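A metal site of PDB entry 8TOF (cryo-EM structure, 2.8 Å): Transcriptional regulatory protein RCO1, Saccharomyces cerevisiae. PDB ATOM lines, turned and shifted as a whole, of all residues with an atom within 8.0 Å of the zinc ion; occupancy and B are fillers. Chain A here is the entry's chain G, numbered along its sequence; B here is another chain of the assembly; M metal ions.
The backbone carbonyl oxygen (O) of Cys 263 sits close to the side-chain amide oxygen (OD1) of Asn 267, at 3.3 Å. SG of Cys 263 sits close to N of Ala 265 (3.3 Å). The side-chain amide oxygen (OE1) of Gln 350 sits close to the backbone carbonyl oxygen (O) of Cys 266 (3.3 Å). The backbone NH of Cys 263 is in hydrogen-bond range of the backbone carbonyl oxygen of Gln 268. SG of Cys 266 sits close to NE of Arg 300 of chain B, at 3.8 Å. The backbone carbonyl oxygen (O) of Cys 286 lies within hydrogen-bond range of the guanidinium group (NH1) of Arg 303 of chain B, at 2.6 Å. NE2 of His 283 sits close to NH2 of Arg 300 of chain B. A ring nitrogen (NE2) of His 283 lies within hydrogen-bond range of the backbone carbonyl oxygen (O) of Ser 269 (3.0 Å).
Of the 23 residues printed, 4 come within 4 Å of the zinc ion.
The zinc ion is bound by a ring nitrogen (ND1) of His 283 (2.0 Å), the side-chain sulfur (SG) of Cys 266 (2.3 Å), the side-chain sulfur (SG) of Cys 263 (2.3 Å) and the side-chain sulfur (SG) of Cys 286 (2.3 Å).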
ATOM      1  N   PHE A 262     -21.254  21.071  22.215  1.00  0.00           N
ATOM      2  CA  PHE A 262     -21.027  19.652  21.972  1.00  0.00           C
ATOM      3  C   PHE A 262     -20.278  19.045  23.150  1.00  0.00           C
ATOM      4  O   PHE A 262     -19.399  19.683  23.741  1.00  0.00           O
ATOM      5  CB  PHE A 262     -20.240  19.425  20.681  1.00  0.00           C
ATOM      6  CG  PHE A 262     -21.114  19.176  19.482  1.00  0.00           C
ATOM      7  CD1 PHE A 262     -22.030  20.123  19.075  1.00  0.00           C
ATOM      8  CD2 PHE A 262     -21.006  18.000  18.760  1.00  0.00           C
ATOM      9  CE1 PHE A 262     -22.830  19.910  17.974  1.00  0.00           C
ATOM     10  CE2 PHE A 262     -21.798  17.776  17.663  1.00  0.00           C
ATOM     11  CZ  PHE A 262     -22.719  18.732  17.265  1.00  0.00           C
ATOM     12  N   CYS A 263     -20.609  17.797  23.474  1.00  0.00           N
ATOM     13  CA  CYS A 263     -19.974  17.132  24.598  1.00  0.00           C
ATOM     14  C   CYS A 263     -18.492  16.913  24.291  1.00  0.00           C
ATOM     15  O   CYS A 263     -18.152  16.240  23.318  1.00  0.00           O
ATOM     16  CB  CYS A 263     -20.655  15.796  24.894  1.00  0.00           C
ATOM     17  SG  CYS A 263     -19.733  14.759  26.039  1.00  0.00           S
ATOM     18  N   SER A 264     -17.634  17.458  25.139  1.00  0.00           N
ATOM     19  CA  SER A 264     -16.195  17.426  24.898  1.00  0.00           C
ATOM     20  C   SER A 264     -15.642  16.024  25.023  1.00  0.00           C
ATOM     21  O   SER A 264     -14.496  15.772  24.640  1.00  0.00           O
ATOM     22  CB  SER A 264     -15.484  18.371  25.863  1.00  0.00           C
ATOM     23  OG  SER A 264     -16.176  19.596  25.997  1.00  0.00           O
ATOM     24  N   ALA A 265     -16.437  15.095  25.554  1.00  0.00           N
ATOM     25  CA  ALA A 265     -15.999  13.721  25.772  1.00  0.00           C
ATOM     26  C   ALA A 265     -16.346  12.803  24.615  1.00  0.00           C
ATOM     27  O   ALA A 265     -15.486  12.053  24.139  1.00  0.00           O
ATOM     28  CB  ALA A 265     -16.604  13.183  27.067  1.00  0.00           C
ATOM     29  N   CYS A 266     -17.592  12.840  24.145  1.00  0.00           N
ATOM     30  CA  CYS A 266     -18.021  12.024  23.024  1.00  0.00           C
ATOM     31  C   CYS A 266     -18.283  12.832  21.755  1.00  0.00           C
ATOM     32  O   CYS A 266     -18.585  12.232  20.717  1.00  0.00           O
ATOM     33  CB  CYS A 266     -19.281  11.228  23.393  1.00  0.00           C
ATOM     34  SG  CYS A 266     -20.809  12.175  23.364  1.00  0.00           S
ATOM     35  N   ASN A 267     -18.163  14.158  21.812  1.00  0.00           N
ATOM     36  CA  ASN A 267     -18.315  15.011  20.641  1.00  0.00           C
ATOM     37  C   ASN A 267     -19.690  14.809  19.992  1.00  0.00           C
ATOM     38  O   ASN A 267     -19.821  14.412  18.836  1.00  0.00           O
ATOM     39  CB  ASN A 267     -17.194  14.749  19.622  1.00  0.00           C
ATOM     40  CG  ASN A 267     -15.824  14.781  20.247  1.00  0.00           C
ATOM     41  OD1 ASN A 267     -15.662  15.176  21.410  1.00  0.00           O
ATOM     42  ND2 ASN A 267     -14.811  14.381  19.484  1.00  0.00           N
ATOM     43  N   GLN A 268     -20.722  15.098  20.783  1.00  0.00           N
ATOM     44  CA  GLN A 268     -22.096  14.990  20.319  1.00  0.00           C
ATOM     45  C   GLN A 268     -22.947  15.970  21.123  1.00  0.00           C
ATOM     46  O   GLN A 268     -22.445  16.684  21.999  1.00  0.00           O
ATOM     47  CB  GLN A 268     -22.608  13.559  20.445  1.00  0.00           C
ATOM     48  CG  GLN A 268     -21.825  12.557  19.595  1.00  0.00           C
ATOM     49  CD  GLN A 268     -22.445  11.186  19.583  1.00  0.00           C
ATOM     50  OE1 GLN A 268     -23.660  11.036  19.684  1.00  0.00           O
ATOM     51  NE2 GLN A 268     -21.605  10.162  19.461  1.00  0.00           N
ATOM     52  N   SER A 269     -24.240  16.015  20.802  1.00  0.00           N
ATOM     53  CA  SER A 269     -25.152  16.992  21.364  1.00  0.00           C
ATOM     54  C   SER A 269     -26.045  16.362  22.421  1.00  0.00           C
ATOM     55  O   SER A 269     -26.249  15.153  22.460  1.00  0.00           O
ATOM     56  CB  SER A 269     -26.008  17.608  20.262  1.00  0.00           C
ATOM     57  OG  SER A 269     -26.454  16.612  19.358  1.00  0.00           O
ATOM     58  N   GLY A 270     -26.583  17.217  23.289  1.00  0.00           N
ATOM     59  CA  GLY A 270     -27.472  16.759  24.334  1.00  0.00           C
ATOM     60  C   GLY A 270     -27.461  17.726  25.503  1.00  0.00           C
ATOM     61  O   GLY A 270     -26.862  18.803  25.438  1.00  0.00           O
ATOM     62  N   SER A 271     -28.125  17.312  26.577  1.00  0.00           N
ATOM     63  CA  SER A 271     -28.116  18.082  27.806  1.00  0.00           C
ATOM     64  C   SER A 271     -26.712  18.096  28.392  1.00  0.00           C
ATOM     65  O   SER A 271     -25.983  17.104  28.319  1.00  0.00           O
ATOM     66  CB  SER A 271     -29.112  17.513  28.811  1.00  0.00           C
ATOM     67  OG  SER A 271     -30.360  18.167  28.720  1.00  0.00           O
ATOM     68  N   PHE A 272     -26.344  19.227  28.978  1.00  0.00           N
ATOM     69  CA  PHE A 272     -24.968  19.439  29.402  1.00  0.00           C
ATOM     70  C   PHE A 272     -24.909  20.060  30.786  1.00  0.00           C
ATOM     71  O   PHE A 272     -25.743  20.912  31.129  1.00  0.00           O
ATOM     72  CB  PHE A 272     -24.222  20.342  28.421  1.00  0.00           C
ATOM     73  CG  PHE A 272     -24.150  19.794  27.031  1.00  0.00           C
ATOM     74  CD1 PHE A 272     -23.728  18.493  26.802  1.00  0.00           C
ATOM     75  CD2 PHE A 272     -24.496  20.580  25.945  1.00  0.00           C
ATOM     76  CE1 PHE A 272     -23.659  17.985  25.519  1.00  0.00           C
ATOM     77  CE2 PHE A 272     -24.427  20.082  24.663  1.00  0.00           C
ATOM     78  CZ  PHE A 272     -24.002  18.779  24.448  1.00  0.00           C
ATOM     79  N   SER A 281     -17.815  21.395  27.792  1.00  0.00           N
ATOM     80  CA  SER A 281     -19.126  20.910  28.205  1.00  0.00           C
ATOM     81  C   SER A 281     -19.190  19.403  28.008  1.00  0.00           C
ATOM     82  O   SER A 281     -18.591  18.872  27.066  1.00  0.00           O
ATOM     83  CB  SER A 281     -20.236  21.602  27.419  1.00  0.00           C
ATOM     84  OG  SER A 281     -21.450  20.888  27.525  1.00  0.00           O
ATOM     85  N   PHE A 282     -19.928  18.740  28.889  1.00  0.00           N
ATOM     86  CA  PHE A 282     -20.039  17.279  28.867  1.00  0.00           C
ATOM     87  C   PHE A 282     -21.498  16.867  29.021  1.00  0.00           C
ATOM     88  O   PHE A 282     -22.329  17.623  29.528  1.00  0.00           O
ATOM     89  CB  PHE A 282     -19.222  16.634  29.990  1.00  0.00           C
ATOM     90  CG  PHE A 282     -17.759  16.898  29.913  1.00  0.00           C
ATOM     91  CD1 PHE A 282     -16.941  16.086  29.156  1.00  0.00           C
ATOM     92  CD2 PHE A 282     -17.202  17.946  30.617  1.00  0.00           C
ATOM     93  CE1 PHE A 282     -15.587  16.326  29.079  1.00  0.00           C
ATOM     94  CE2 PHE A 282     -15.845  18.185  30.554  1.00  0.00           C
ATOM     95  CZ  PHE A 282     -15.045  17.375  29.786  1.00  0.00           C
ATOM     96  N   HIS A 283     -21.792  15.648  28.584  1.00  0.00           N
ATOM     97  CA  HIS A 283     -23.043  15.024  28.933  1.00  0.00           C
ATOM     98  C   HIS A 283     -23.047  14.693  30.426  1.00  0.00           C
ATOM     99  O   HIS A 283     -22.042  14.832  31.119  1.00  0.00           O
ATOM    100  CB  HIS A 283     -23.264  13.756  28.112  1.00  0.00           C
ATOM    101  CG  HIS A 283     -23.591  14.020  26.676  1.00  0.00           C
ATOM    102  ND1 HIS A 283     -22.868  13.460  25.646  1.00  0.00           N
ATOM    103  CD2 HIS A 283     -24.543  14.783  26.104  1.00  0.00           C
ATOM    104  CE1 HIS A 283     -23.368  13.859  24.487  1.00  0.00           C
ATOM    105  NE2 HIS A 283     -24.390  14.660  24.742  1.00  0.00           N
ATOM    106  N   PHE A 284     -24.201  14.262  30.920  1.00  0.00           N
ATOM    107  CA  PHE A 284     -24.277  13.815  32.300  1.00  0.00           C
ATOM    108  C   PHE A 284     -23.811  12.375  32.461  1.00  0.00           C
ATOM    109  O   PHE A 284     -23.327  12.004  33.539  1.00  0.00           O
ATOM    110  CB  PHE A 284     -25.715  13.961  32.821  1.00  0.00           C
ATOM    111  CG  PHE A 284     -26.180  15.380  32.898  1.00  0.00           C
ATOM    112  CD1 PHE A 284     -26.536  16.061  31.752  1.00  0.00           C
ATOM    113  CD2 PHE A 284     -26.245  16.025  34.107  1.00  0.00           C
ATOM    114  CE1 PHE A 284     -26.958  17.377  31.816  1.00  0.00           C
ATOM    115  CE2 PHE A 284     -26.672  17.341  34.179  1.00  0.00           C
ATOM    116  CZ  PHE A 284     -27.029  18.012  33.033  1.00  0.00           C
ATOM    117  N   LEU A 285     -23.933  11.554  31.418  1.00  0.00           N
ATOM    118  CA  LEU A 285     -23.480  10.177  31.444  1.00  0.00           C
ATOM    119  C   LEU A 285     -22.100  10.023  30.825  1.00  0.00           C
ATOM    120  O   LEU A 285     -21.609   8.891  30.686  1.00  0.00           O
ATOM    121  CB  LEU A 285     -24.497   9.287  30.725  1.00  0.00           C
ATOM    122  CG  LEU A 285     -24.438   7.801  31.085  1.00  0.00           C
ATOM    123  CD1 LEU A 285     -25.203   7.535  32.364  1.00  0.00           C
ATOM    124  CD2 LEU A 285     -24.999   6.963  29.961  1.00  0.00           C
ATOM    125  N   CYS A 286     -21.462  11.129  30.441  1.00  0.00           N
ATOM    126  CA  CYS A 286     -20.103  11.107  29.935  1.00  0.00           C
ATOM    127  C   CYS A 286     -19.080  11.596  30.944  1.00  0.00           C
ATOM    128  O   CYS A 286     -17.871  11.448  30.704  1.00  0.00           O
ATOM    129  CB  CYS A 286     -19.988  11.953  28.662  1.00  0.00           C
ATOM    130  SG  CYS A 286     -20.602  11.154  27.160  1.00  0.00           S
ATOM    131  N   LEU A 287     -19.508  12.150  32.070  1.00  0.00           N
ATOM    132  CA  LEU A 287     -18.588  12.572  33.116  1.00  0.00           C
ATOM    133  C   LEU A 287     -18.035  11.346  33.834  1.00  0.00           C
ATOM    134  O   LEU A 287     -18.305  10.199  33.465  1.00  0.00           O
ATOM    135  CB  LEU A 287     -19.280  13.517  34.093  1.00  0.00           C
ATOM    136  CG  LEU A 287     -19.624  14.896  33.543  1.00  0.00           C
ATOM    137  CD1 LEU A 287     -20.496  15.650  34.523  1.00  0.00           C
ATOM    138  CD2 LEU A 287     -18.360  15.687  33.223  1.00  0.00           C
ATOM    139  N   PRO A 348     -12.744  13.123  30.999  1.00  0.00           N
ATOM    140  CA  PRO A 348     -13.183  11.869  30.372  1.00  0.00           C
ATOM    141  C   PRO A 348     -13.276  12.025  28.866  1.00  0.00           C
ATOM    142  O   PRO A 348     -13.631  13.090  28.351  1.00  0.00           O
ATOM    143  CB  PRO A 348     -14.555  11.619  30.997  1.00  0.00           C
ATOM    144  CG  PRO A 348     -14.576  12.429  32.244  1.00  0.00           C
ATOM    145  CD  PRO A 348     -13.755  13.636  31.948  1.00  0.00           C
ATOM    146  N   GLN A 350     -14.413   9.766  25.228  1.00  0.00           N
ATOM    147  CA  GLN A 350     -14.976   8.568  24.619  1.00  0.00           C
ATOM    148  C   GLN A 350     -13.882   7.787  23.900  1.00  0.00           C
ATOM    149  O   GLN A 350     -12.988   8.376  23.283  1.00  0.00           O
ATOM    150  CB  GLN A 350     -16.083   8.946  23.639  1.00  0.00           C
ATOM    151  CG  GLN A 350     -16.916   7.793  23.144  1.00  0.00           C
ATOM    152  CD  GLN A 350     -17.394   7.994  21.727  1.00  0.00           C
ATOM    153  OE1 GLN A 350     -17.983   9.024  21.403  1.00  0.00           O
ATOM    154  NE2 GLN A 350     -17.163   7.014  20.867  1.00  0.00           N
ATOM    155  N   ARG B 300     -19.714   5.506  23.962  1.00  0.00           N
ATOM    156  CA  ARG B 300     -20.812   6.193  24.614  1.00  0.00           C
ATOM    157  C   ARG B 300     -21.890   5.209  25.054  1.00  0.00           C
ATOM    158  O   ARG B 300     -22.523   5.399  26.098  1.00  0.00           O
ATOM    159  CB  ARG B 300     -21.406   7.258  23.706  1.00  0.00           C
ATOM    160  CG  ARG B 300     -22.406   8.146  24.408  1.00  0.00           C
ATOM    161  CD  ARG B 300     -23.103   9.081  23.450  1.00  0.00           C
ATOM    162  NE  ARG B 300     -23.879  10.087  24.161  1.00  0.00           N
ATOM    163  CZ  ARG B 300     -24.785  10.876  23.596  1.00  0.00           C
ATOM    164  NH1 ARG B 300     -25.050  10.812  22.301  1.00  0.00           N
ATOM    165  NH2 ARG B 300     -25.455  11.730  24.355  1.00  0.00           N
ATOM    166  N   ARG B 303     -21.301   3.484  28.497  1.00  0.00           N
ATOM    167  CA  ARG B 303     -21.204   4.367  29.646  1.00  0.00           C
ATOM    168  C   ARG B 303     -22.468   4.372  30.486  1.00  0.00           C
ATOM    169  O   ARG B 303     -22.551   5.121  31.463  1.00  0.00           O
ATOM    170  CB  ARG B 303     -20.844   5.776  29.194  1.00  0.00           C
ATOM    171  CG  ARG B 303     -19.372   5.935  28.843  1.00  0.00           C
ATOM    172  CD  ARG B 303     -18.759   7.181  29.440  1.00  0.00           C
ATOM    173  NE  ARG B 303     -17.864   6.865  30.537  1.00  0.00           N
ATOM    174  CZ  ARG B 303     -17.520   7.711  31.498  1.00  0.00           C
ATOM    175  NH1 ARG B 303     -17.983   8.943  31.517  1.00  0.00           N
ATOM    176  NH2 ARG B 303     -16.701   7.312  32.457  1.00  0.00           N
ATOM    177  N   ALA B 398     -28.756   5.831  27.102  1.00  0.00           N
ATOM    178  CA  ALA B 398     -27.319   5.872  26.840  1.00  0.00           C
ATOM    179  C   ALA B 398     -26.987   6.909  25.766  1.00  0.00           C
ATOM    180  O   ALA B 398     -26.022   7.664  25.907  1.00  0.00           O
ATOM    181  CB  ALA B 398     -26.819   4.494  26.419  1.00  0.00           C
HETATM  182 ZN    ZN M   1     -20.935  12.830  25.584  1.00  0.00          ZN
